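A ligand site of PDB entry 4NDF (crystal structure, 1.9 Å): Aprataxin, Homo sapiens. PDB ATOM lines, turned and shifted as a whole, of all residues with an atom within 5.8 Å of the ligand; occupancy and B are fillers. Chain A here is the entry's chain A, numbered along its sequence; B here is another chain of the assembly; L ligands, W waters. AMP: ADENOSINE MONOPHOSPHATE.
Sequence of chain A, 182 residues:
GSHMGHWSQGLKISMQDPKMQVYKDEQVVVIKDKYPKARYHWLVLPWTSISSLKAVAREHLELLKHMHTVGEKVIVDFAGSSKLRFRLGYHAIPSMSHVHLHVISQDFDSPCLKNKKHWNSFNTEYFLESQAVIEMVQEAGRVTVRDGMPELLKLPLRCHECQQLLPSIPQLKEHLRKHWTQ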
ATOM      1  N   GLY A  10      17.909  -1.300  13.118  1.00  0.00           N
ATOM      2  CA  GLY A  10      16.898  -2.338  13.280  1.00  0.00           C
ATOM      3  C   GLY A  10      16.974  -3.490  12.283  1.00  0.00           C
ATOM      4  O   GLY A  10      16.653  -4.624  12.637  1.00  0.00           O
ATOM      5  N   LEU A  11      17.385  -3.203  11.054  1.00  0.00           N
ATOM      6  CA  LEU A  11      17.459  -4.233  10.022  1.00  0.00           C
ATOM      7  C   LEU A  11      18.538  -5.254  10.340  1.00  0.00           C
ATOM      8  O   LEU A  11      18.417  -6.436   9.996  1.00  0.00           O
ATOM      9  CB  LEU A  11      17.729  -3.619   8.638  1.00  0.00           C
ATOM     10  CG  LEU A  11      16.658  -2.670   8.088  1.00  0.00           C
ATOM     11  CD1 LEU A  11      17.013  -2.261   6.654  1.00  0.00           C
ATOM     12  CD2 LEU A  11      15.292  -3.308   8.142  1.00  0.00           C
ATOM     13  N   SER A  14      16.770  -7.670  12.597  1.00  0.00           N
ATOM     14  CA  SER A  14      15.746  -8.434  11.869  1.00  0.00           C
ATOM     15  C   SER A  14      16.335  -9.422  10.887  1.00  0.00           C
ATOM     16  O   SER A  14      15.833 -10.545  10.755  1.00  0.00           O
ATOM     17  CB  SER A  14      14.802  -7.487  11.125  1.00  0.00           C
ATOM     18  OG  SER A  14      14.012  -6.763  12.051  1.00  0.00           O
ATOM     19  N   MET A  20      11.644 -13.940  10.714  1.00  0.00           N
ATOM     20  CA  MET A  20      11.452 -12.896   9.728  1.00  0.00           C
ATOM     21  C   MET A  20      12.055 -13.280   8.379  1.00  0.00           C
ATOM     22  O   MET A  20      11.708 -12.716   7.347  1.00  0.00           O
ATOM     23  CB  MET A  20      12.028 -11.570  10.207  1.00  0.00           C
ATOM     24  CG  MET A  20      11.343 -11.037  11.463  1.00  0.00           C
ATOM     25  SD  MET A  20      11.870  -9.373  11.866  1.00  0.00           S
ATOM     26  CE  MET A  20      10.845  -9.043  13.293  1.00  0.00           C
ATOM     27  N   ILE A  31      13.939 -10.809   4.149  1.00  0.00           N
ATOM     28  CA  ILE A  31      13.029 -10.736   5.272  1.00  0.00           C
ATOM     29  C   ILE A  31      11.745 -10.039   4.887  1.00  0.00           C
ATOM     30  O   ILE A  31      11.693  -9.287   3.906  1.00  0.00           O
ATOM     31  CB  ILE A  31      13.651 -10.002   6.478  1.00  0.00           C
ATOM     32  CG1 ILE A  31      13.984  -8.558   6.117  1.00  0.00           C
ATOM     33  CG2 ILE A  31      14.896 -10.741   6.994  1.00  0.00           C
ATOM     34  CD1 ILE A  31      14.518  -7.776   7.296  1.00  0.00           C
ATOM     35  N   LYS A  32      10.693 -10.294   5.650  1.00  0.00           N
ATOM     36  CA  LYS A  32       9.470  -9.510   5.497  1.00  0.00           C
ATOM     37  C   LYS A  32       9.732  -8.093   6.006  1.00  0.00           C
ATOM     38  O   LYS A  32      10.361  -7.925   7.050  1.00  0.00           O
ATOM     39  CB  LYS A  32       8.339 -10.181   6.266  1.00  0.00           C
ATOM     40  CG  LYS A  32       7.940 -11.525   5.682  1.00  0.00           C
ATOM     41  CD  LYS A  32       6.656 -12.040   6.311  1.00  0.00           C
ATOM     42  CE  LYS A  32       6.875 -12.548   7.708  1.00  0.00           C
ATOM     43  NZ  LYS A  32       5.638 -13.116   8.333  1.00  0.00           N
ATOM     44  N   ASP A  33       9.292  -7.091   5.263  1.00  0.00           N
ATOM     45  CA  ASP A  33       9.310  -5.726   5.766  1.00  0.00           C
ATOM     46  C   ASP A  33       8.410  -5.689   7.008  1.00  0.00           C
ATOM     47  O   ASP A  33       7.300  -6.212   7.002  1.00  0.00           O
ATOM     48  CB  ASP A  33       8.802  -4.739   4.714  1.00  0.00           C
ATOM     49  CG  ASP A  33       9.132  -3.280   5.063  1.00  0.00           C
ATOM     50  OD1 ASP A  33       8.501  -2.739   5.999  1.00  0.00           O
ATOM     51  OD2 ASP A  33      10.001  -2.675   4.407  1.00  0.00           O
ATOM     52  N   LYS A  34       8.909  -5.082   8.082  1.00  0.00           N
ATOM     53  CA  LYS A  34       8.181  -5.037   9.340  1.00  0.00           C
ATOM     54  C   LYS A  34       6.918  -4.153   9.292  1.00  0.00           C
ATOM     55  O   LYS A  34       5.961  -4.344  10.056  1.00  0.00           O
ATOM     56  CB  LYS A  34       9.104  -4.561  10.450  1.00  0.00           C
ATOM     57  CG  LYS A  34       8.474  -4.578  11.834  1.00  0.00           C
ATOM     58  CD  LYS A  34       9.494  -4.268  12.905  1.00  0.00           C
ATOM     59  CE  LYS A  34       8.871  -4.335  14.277  1.00  0.00           C
ATOM     60  NZ  LYS A  34       9.886  -4.095  15.326  1.00  0.00           N
ATOM     61  N   TYR A  35       6.935  -3.169   8.408  1.00  0.00           N
ATOM     62  CA  TYR A  35       5.799  -2.279   8.217  1.00  0.00           C
ATOM     63  C   TYR A  35       5.456  -2.230   6.745  1.00  0.00           C
ATOM     64  O   TYR A  35       5.633  -1.195   6.100  1.00  0.00           O
ATOM     65  CB  TYR A  35       6.130  -0.876   8.714  1.00  0.00           C
ATOM     66  CG  TYR A  35       6.657  -0.855  10.125  1.00  0.00           C
ATOM     67  CD1 TYR A  35       5.789  -0.884  11.214  1.00  0.00           C
ATOM     68  CD2 TYR A  35       8.018  -0.830  10.377  1.00  0.00           C
ATOM     69  CE1 TYR A  35       6.262  -0.875  12.505  1.00  0.00           C
ATOM     70  CE2 TYR A  35       8.501  -0.832  11.668  1.00  0.00           C
ATOM     71  CZ  TYR A  35       7.623  -0.849  12.727  1.00  0.00           C
ATOM     72  OH  TYR A  35       8.116  -0.841  14.018  1.00  0.00           O
ATOM     73  N   PRO A  36       4.953  -3.358   6.201  1.00  0.00           N
ATOM     74  CA  PRO A  36       4.828  -3.506   4.757  1.00  0.00           C
ATOM     75  C   PRO A  36       3.894  -2.456   4.177  1.00  0.00           C
ATOM     76  O   PRO A  36       2.868  -2.145   4.782  1.00  0.00           O
ATOM     77  CB  PRO A  36       4.234  -4.923   4.605  1.00  0.00           C
ATOM     78  CG  PRO A  36       3.535  -5.193   5.911  1.00  0.00           C
ATOM     79  CD  PRO A  36       4.428  -4.532   6.938  1.00  0.00           C
ATOM     80  N   LYS A  37       4.267  -1.888   3.030  1.00  0.00           N
ATOM     81  CA  LYS A  37       3.454  -0.825   2.418  1.00  0.00           C
ATOM     82  C   LYS A  37       2.597  -1.364   1.284  1.00  0.00           C
ATOM     83  O   LYS A  37       2.020  -0.592   0.496  1.00  0.00           O
ATOM     84  CB  LYS A  37       4.355   0.323   1.942  1.00  0.00           C
ATOM     85  CG  LYS A  37       5.255   0.921   3.027  1.00  0.00           C
ATOM     86  CD  LYS A  37       4.437   1.437   4.215  1.00  0.00           C
ATOM     87  CE  LYS A  37       5.291   2.274   5.170  1.00  0.00           C
ATOM     88  NZ  LYS A  37       6.436   1.518   5.787  1.00  0.00           N
ATOM     89  N   HIS A  41       5.708  -7.289   0.658  1.00  0.00           N
ATOM     90  CA  HIS A  41       6.791  -6.328   0.802  1.00  0.00           C
ATOM     91  C   HIS A  41       7.933  -7.017   1.512  1.00  0.00           C
ATOM     92  O   HIS A  41       7.862  -7.307   2.713  1.00  0.00           O
ATOM     93  CB  HIS A  41       6.314  -5.099   1.591  1.00  0.00           C
ATOM     94  CG  HIS A  41       7.256  -3.930   1.525  1.00  0.00           C
ATOM     95  ND1 HIS A  41       6.994  -2.730   2.138  1.00  0.00           N
ATOM     96  CD2 HIS A  41       8.465  -3.792   0.924  1.00  0.00           C
ATOM     97  CE1 HIS A  41       7.990  -1.889   1.918  1.00  0.00           C
ATOM     98  NE2 HIS A  41       8.902  -2.508   1.184  1.00  0.00           N
ATOM     99  N   LEU A  43      12.405  -7.319   1.954  1.00  0.00           N
ATOM    100  CA  LEU A  43      13.702  -6.654   1.842  1.00  0.00           C
ATOM    101  C   LEU A  43      14.765  -7.724   1.627  1.00  0.00           C
ATOM    102  O   LEU A  43      14.793  -8.726   2.339  1.00  0.00           O
ATOM    103  CB  LEU A  43      14.018  -5.881   3.126  1.00  0.00           C
ATOM    104  CG  LEU A  43      13.020  -4.803   3.549  1.00  0.00           C
ATOM    105  CD1 LEU A  43      13.438  -4.170   4.886  1.00  0.00           C
ATOM    106  CD2 LEU A  43      12.857  -3.738   2.443  1.00  0.00           C
ATOM    107  N   HIS A  91      15.253   3.153  -2.108  1.00  0.00           N
ATOM    108  CA  HIS A  91      14.926   4.540  -1.817  1.00  0.00           C
ATOM    109  C   HIS A  91      16.163   5.394  -2.031  1.00  0.00           C
ATOM    110  O   HIS A  91      17.250   5.010  -1.609  1.00  0.00           O
ATOM    111  CB  HIS A  91      14.419   4.683  -0.379  1.00  0.00           C
ATOM    112  CG  HIS A  91      13.008   4.224  -0.186  1.00  0.00           C
ATOM    113  ND1 HIS A  91      12.461   3.996   1.058  1.00  0.00           N
ATOM    114  CD2 HIS A  91      12.025   3.956  -1.086  1.00  0.00           C
ATOM    115  CE1 HIS A  91      11.198   3.619   0.920  1.00  0.00           C
ATOM    116  NE2 HIS A  91      10.914   3.586  -0.366  1.00  0.00           N
ATOM    117  N   ILE A  93      17.146   8.094  -0.717  1.00  0.00           N
ATOM    118  CA  ILE A  93      17.729   8.376   0.582  1.00  0.00           C
ATOM    119  C   ILE A  93      17.055   7.434   1.572  1.00  0.00           C
ATOM    120  O   ILE A  93      15.883   7.615   1.904  1.00  0.00           O
ATOM    121  CB  ILE A  93      17.501   9.851   1.024  1.00  0.00           C
ATOM    122  CG1 ILE A  93      17.994  10.819  -0.060  1.00  0.00           C
ATOM    123  CG2 ILE A  93      18.205  10.143   2.342  1.00  0.00           C
ATOM    124  CD1 ILE A  93      17.743  12.289   0.262  1.00  0.00           C
ATOM    125  N   PRO A  94      17.766   6.394   2.027  1.00  0.00           N
ATOM    126  CA  PRO A  94      17.184   5.477   2.995  1.00  0.00           C
ATOM    127  C   PRO A  94      17.189   6.066   4.399  1.00  0.00           C
ATOM    128  O   PRO A  94      17.827   7.085   4.655  1.00  0.00           O
ATOM    129  CB  PRO A  94      18.110   4.259   2.938  1.00  0.00           C
ATOM    130  CG  PRO A  94      19.435   4.841   2.571  1.00  0.00           C
ATOM    131  CD  PRO A  94      19.131   5.982   1.621  1.00  0.00           C
ATOM    132  N   SER A  95      16.473   5.411   5.310  1.00  0.00           N
ATOM    133  CA  SER A  95      16.503   5.788   6.715  1.00  0.00           C
ATOM    134  C   SER A  95      17.241   4.723   7.529  1.00  0.00           C
ATOM    135  O   SER A  95      17.938   5.029   8.497  1.00  0.00           O
ATOM    136  CB  SER A  95      15.074   5.950   7.243  1.00  0.00           C
ATOM    137  OG  SER A  95      14.390   7.005   6.597  1.00  0.00           O
ATOM    138  N   MET A  96      17.073   3.465   7.134  1.00  0.00           N
ATOM    139  CA  MET A  96      17.646   2.354   7.879  1.00  0.00           C
ATOM    140  C   MET A  96      19.008   1.957   7.324  1.00  0.00           C
ATOM    141  O   MET A  96      19.176   1.900   6.117  1.00  0.00           O
ATOM    142  CB  MET A  96      16.698   1.149   7.823  1.00  0.00           C
ATOM    143  CG  MET A  96      15.306   1.406   8.404  1.00  0.00           C
ATOM    144  SD  MET A  96      15.280   1.704  10.178  1.00  0.00           S
ATOM    145  CE  MET A  96      15.712   0.066  10.786  1.00  0.00           C
ATOM    146  N   HIS A 100      19.689  -2.478   1.433  1.00  0.00           N
ATOM    147  CA  HIS A 100      18.542  -3.367   1.354  1.00  0.00           C
ATOM    148  C   HIS A 100      17.713  -3.042   0.123  1.00  0.00           C
ATOM    149  O   HIS A 100      17.437  -1.868  -0.166  1.00  0.00           O
ATOM    150  CB  HIS A 100      17.686  -3.283   2.626  1.00  0.00           C
ATOM    151  CG  HIS A 100      17.282  -1.884   2.989  1.00  0.00           C
ATOM    152  ND1 HIS A 100      18.091  -1.024   3.696  1.00  0.00           N
ATOM    153  CD2 HIS A 100      16.129  -1.211   2.750  1.00  0.00           C
ATOM    154  CE1 HIS A 100      17.463   0.117   3.883  1.00  0.00           C
ATOM    155  NE2 HIS A 100      16.271   0.042   3.316  1.00  0.00           N
ATOM    156  N   HIS A 102      14.216  -3.195  -1.800  1.00  0.00           N
ATOM    157  CA  HIS A 102      12.765  -3.338  -1.674  1.00  0.00           C
ATOM    158  C   HIS A 102      12.196  -4.199  -2.806  1.00  0.00           C
ATOM    159  O   HIS A 102      12.523  -3.998  -3.966  1.00  0.00           O
ATOM    160  CB  HIS A 102      12.099  -1.955  -1.706  1.00  0.00           C
ATOM    161  CG  HIS A 102      12.285  -1.162  -0.458  1.00  0.00           C
ATOM    162  ND1 HIS A 102      11.385  -1.197   0.591  1.00  0.00           N
ATOM    163  CD2 HIS A 102      13.258  -0.282  -0.085  1.00  0.00           C
ATOM    164  CE1 HIS A 102      11.805  -0.400   1.563  1.00  0.00           C
ATOM    165  NE2 HIS A 102      12.928   0.167   1.170  1.00  0.00           N
ATOM    166  N   PHE A 122       7.695   5.472  -2.897  1.00  0.00           N
ATOM    167  CA  PHE A 122       7.582   4.309  -3.780  1.00  0.00           C
ATOM    168  C   PHE A 122       7.082   4.657  -5.167  1.00  0.00           C
ATOM    169  O   PHE A 122       7.121   3.804  -6.061  1.00  0.00           O
ATOM    170  CB  PHE A 122       6.690   3.226  -3.162  1.00  0.00           C
ATOM    171  CG  PHE A 122       7.347   2.486  -2.033  1.00  0.00           C
ATOM    172  CD1 PHE A 122       8.241   1.448  -2.283  1.00  0.00           C
ATOM    173  CD2 PHE A 122       7.093   2.836  -0.713  1.00  0.00           C
ATOM    174  CE1 PHE A 122       8.872   0.783  -1.231  1.00  0.00           C
ATOM    175  CE2 PHE A 122       7.704   2.182   0.330  1.00  0.00           C
ATOM    176  CZ  PHE A 122       8.608   1.145   0.070  1.00  0.00           C
ATOM    177  N   TYR A 126      12.086   9.112  -6.364  1.00  0.00           N
ATOM    178  CA  TYR A 126      12.684   8.752  -5.080  1.00  0.00           C
ATOM    179  C   TYR A 126      12.931   7.237  -5.013  1.00  0.00           C
ATOM    180  O   TYR A 126      13.819   6.787  -4.299  1.00  0.00           O
ATOM    181  CB  TYR A 126      11.747   9.158  -3.963  1.00  0.00           C
ATOM    182  CG  TYR A 126      12.383   9.324  -2.609  1.00  0.00           C
ATOM    183  CD1 TYR A 126      12.870  10.558  -2.202  1.00  0.00           C
ATOM    184  CD2 TYR A 126      12.481   8.260  -1.711  1.00  0.00           C
ATOM    185  CE1 TYR A 126      13.424  10.734  -0.956  1.00  0.00           C
ATOM    186  CE2 TYR A 126      13.044   8.425  -0.456  1.00  0.00           C
ATOM    187  CZ  TYR A 126      13.521   9.672  -0.088  1.00  0.00           C
ATOM    188  OH  TYR A 126      14.067   9.878   1.150  1.00  0.00           O
ATOM    189  OP3   G B   1       8.634   6.389   6.327  1.00  0.00           O
ATOM    190  P     G B   1      10.162   6.885   6.264  1.00  0.00           P
ATOM    191  OP1   G B   1      10.259   8.198   6.933  1.00  0.00           O
ATOM    192  OP2   G B   1      10.593   6.807   4.850  1.00  0.00           O
ATOM    193  O5'   G B   1      11.065   5.887   7.107  1.00  0.00           O
ATOM    194  C5'   G B   1      11.212   4.526   6.741  1.00  0.00           C
ATOM    195  C4'   G B   1      11.252   3.665   7.968  1.00  0.00           C
ATOM    196  O4'   G B   1      12.445   3.974   8.735  1.00  0.00           O
ATOM    197  C3'   G B   1      10.110   3.920   8.943  1.00  0.00           C
ATOM    198  O3'   G B   1       8.939   3.214   8.591  1.00  0.00           O
ATOM    199  C2'   G B   1      10.708   3.538  10.287  1.00  0.00           C
ATOM    200  O2'   G B   1      10.733   2.126  10.442  1.00  0.00           O
ATOM    201  C1'   G B   1      12.140   4.015  10.114  1.00  0.00           C
ATOM    202  N9    G B   1      12.368   5.385  10.603  1.00  0.00           N
ATOM    203  C8    G B   1      12.686   6.474   9.827  1.00  0.00           C
ATOM    204  N7    G B   1      12.880   7.569  10.525  1.00  0.00           N
ATOM    205  C5    G B   1      12.693   7.172  11.836  1.00  0.00           C
ATOM    206  C6    G B   1      12.765   7.925  13.034  1.00  0.00           C
ATOM    207  O6    G B   1      13.053   9.134  13.175  1.00  0.00           O
ATOM    208  N1    G B   1      12.497   7.140  14.151  1.00  0.00           N
ATOM    209  C2    G B   1      12.192   5.809  14.116  1.00  0.00           C
ATOM    210  N2    G B   1      11.960   5.230  15.300  1.00  0.00           N
ATOM    211  N3    G B   1      12.115   5.093  13.009  1.00  0.00           N
ATOM    212  C4    G B   1      12.371   5.828  11.911  1.00  0.00           C
ATOM    213  P    DT B   2       7.496   3.869   8.817  1.00  0.00           P
ATOM    214  OP1  DT B   2       6.505   2.949   8.203  1.00  0.00           O
ATOM    215  OP2  DT B   2       7.485   5.290   8.392  1.00  0.00           O
ATOM    216  O5'  DT B   2       7.313   3.843  10.412  1.00  0.00           O
ATOM    217  C5'  DT B   2       7.376   2.628  11.135  1.00  0.00           C
ATOM    218  C4'  DT B   2       7.324   2.958  12.620  1.00  0.00           C
ATOM    219  O4'  DT B   2       8.517   3.694  12.963  1.00  0.00           O
ATOM    220  C3'  DT B   2       6.174   3.856  13.040  1.00  0.00           C
ATOM    221  O3'  DT B   2       5.055   3.070  13.384  1.00  0.00           O
ATOM    222  C2'  DT B   2       6.733   4.534  14.275  1.00  0.00           C
ATOM    223  C1'  DT B   2       8.216   4.620  13.986  1.00  0.00           C
ATOM    224  N1   DT B   2       8.632   5.980  13.579  1.00  0.00           N
ATOM    225  C2   DT B   2       8.899   6.877  14.579  1.00  0.00           C
ATOM    226  O2   DT B   2       8.787   6.591  15.761  1.00  0.00           O
ATOM    227  N3   DT B   2       9.305   8.108  14.147  1.00  0.00           N
ATOM    228  C4   DT B   2       9.442   8.508  12.838  1.00  0.00           C
ATOM    229  O4   DT B   2       9.815   9.646  12.563  1.00  0.00           O
ATOM    230  C5   DT B   2       9.148   7.523  11.825  1.00  0.00           C
ATOM    231  C7   DT B   2       9.278   7.879  10.375  1.00  0.00           C
ATOM    232  C6   DT B   2       8.742   6.303  12.238  1.00  0.00           C
HETATM  233  P   AMP L   1      14.253   2.832   3.867  1.00  0.00           P
HETATM  234  O1P AMP L   1      13.659   4.127   3.359  1.00  0.00           O
HETATM  235  O2P AMP L   1      15.370   2.977   4.870  1.00  0.00           O
HETATM  236  O3P AMP L   1      14.507   1.810   2.811  1.00  0.00           O
HETATM  237  O5' AMP L   1      13.040   2.255   4.722  1.00  0.00           O
HETATM  238  C5' AMP L   1      13.229   1.194   5.648  1.00  0.00           C
HETATM  239  C4' AMP L   1      12.261   0.057   5.405  1.00  0.00           C
HETATM  240  O4' AMP L   1      12.476  -0.958   6.412  1.00  0.00           O
HETATM  241  C3' AMP L   1      10.785   0.440   5.461  1.00  0.00           C
HETATM  242  O3' AMP L   1      10.101  -0.235   4.409  1.00  0.00           O
HETATM  243  C2' AMP L   1      10.331  -0.080   6.842  1.00  0.00           C
HETATM  244  O2' AMP L   1       8.973  -0.458   6.897  1.00  0.00           O
HETATM  245  C1' AMP L   1      11.256  -1.277   7.047  1.00  0.00           C
HETATM  246  N9  AMP L   1      11.610  -1.564   8.439  1.00  0.00           N
HETATM  247  C8  AMP L   1      11.806  -0.682   9.430  1.00  0.00           C
HETATM  248  N7  AMP L   1      12.210  -1.323  10.548  1.00  0.00           N
HETATM  249  C5  AMP L   1      12.301  -2.643  10.265  1.00  0.00           C
HETATM  250  C6  AMP L   1      12.674  -3.870  10.990  1.00  0.00           C
HETATM  251  N6  AMP L   1      13.050  -3.835  12.305  1.00  0.00           N
HETATM  252  N1  AMP L   1      12.617  -5.035  10.316  1.00  0.00           N
HETATM  253  C2  AMP L   1      12.251  -5.092   9.020  1.00  0.00           C
HETATM  254  N3  AMP L   1      11.907  -4.018   8.308  1.00  0.00           N
HETATM  255  C4  AMP L   1      11.906  -2.784   8.866  1.00  0.00           C
HETATM  256  O   HOH W   1      15.838   1.778   0.329  1.00  0.00           O
HETATM  257  O   HOH W   2      14.631  -4.814  14.595  1.00  0.00           O
HETATM  258  O   HOH W   3      13.250   6.373   4.436  1.00  0.00           O
HETATM  259  O   HOH W   4       8.400   1.895   3.787  1.00  0.00           O
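OD2 of Asp 33 lies within hydrogen-bond range of O3' of the ligand, at 2.4 Å. NE2 of His 100 sits at hydrogen-bond distance from O3P of the ligand (2.5 Å). The backbone NH (N) of Met 96 is in hydrogen-bond range of an oxygen (O2P) of the ligand (2.9 Å). N of Lys 34 sits at hydrogen-bond distance from N3 of the ligand. O3P of the ligand sits at hydrogen-bond distance from NE2 of His 102, 2.8 Å away. O1P of the ligand lies within hydrogen-bond range of ND1 of His 91. OG of Ser 14 lies within hydrogen-bond range of N1 of the ligand. N of Ser 95 sits at hydrogen-bond distance from O2P of the ligand, 2.7 Å away. The side-chain amino group of Lys 37 lies within hydrogen-bond range of an oxygen (O2') of the ligand, at 3.4 Å.
A ring nitrogen (ND1) of His 41 is in hydrogen-bond range of the backbone NH (N) of Lys 37 (3.0 Å). The side-chain amino group (NZ) of Lys 37 is in salt-bridge range of OP1 of DT 2 of chain B. O of Met 20 lies within hydrogen-bond range of N of Lys 32 (3.1 Å). The backbone carbonyl oxygen (O) of Ile 31 lies within hydrogen-bond range of the backbone NH (N) of Leu 43, 2.9 Å away. N of Tyr 35 lies within hydrogen-bond range of OD1 of Asp 33, at 2.9 Å. The backbone carbonyl oxygen (O) of His 41 sits at hydrogen-bond distance from the backbone NH (N) of Asp 33, at 2.9 Å. ND1 of His 102 is in hydrogen-bond range of NE2 of His 41 (2.9 Å). The side-chain hydroxyl (OG) of Ser 14 sits at hydrogen-bond distance from the backbone carbonyl oxygen (O) of Gly 10.
O of Gly 10 touches N6 of the ligand, 3.7 Å away. Leu 11 touches the ligand (CD2 to N3, 3.5 Å). CD1 of Ile 31 touches C2 of the ligand, at 3.9 Å. Lys 32 touches the ligand (O to C2, 3.9 Å). Tyr 35 touches the ligand (CB to O2', 3.4 Å). His 41 touches the ligand. CD1 of Leu 43 touches O4' of the ligand (3.7 Å). Pro 94 touches the ligand (CB to O2P, 3.6 Å). G 1 of chain B touches the ligand. 18 residues have an atom within 4 Å of the ligand: Gly 10, Leu 11, Ser 14, Ile 31, Lys 32, Asp 33, Lys 34, Tyr 35, Lys 37, His 41, Leu 43, His 91, Pro 94, Ser 95, Met 96, His 100, His 102 and G 1 of chain B.
Water W3 lies within hydrogen-bond range of an oxygen (O1P) of the ligand (2.5 Å), the side-chain hydroxyl (OG) of Ser 95 (2.5 Å) and OP2 of G 1 of chain B (2.7 Å). Water W4 lies within hydrogen-bond range of O3' of the ligand and NZ of Lys 37. Water W1 lies within hydrogen-bond range of an oxygen (O3P) of the ligand, the backbone NH of His 91, a ring nitrogen (NE2) of His 102 and a ring nitrogen (NE2) of His 100. Water W2 lies within hydrogen-bond range of the backbone carbonyl oxygen of Gly 10 (2.8 Å), a nitrogen (N6) of the ligand (2.9 Å) and the side-chain hydroxyl of Ser 14 (3.3 Å).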
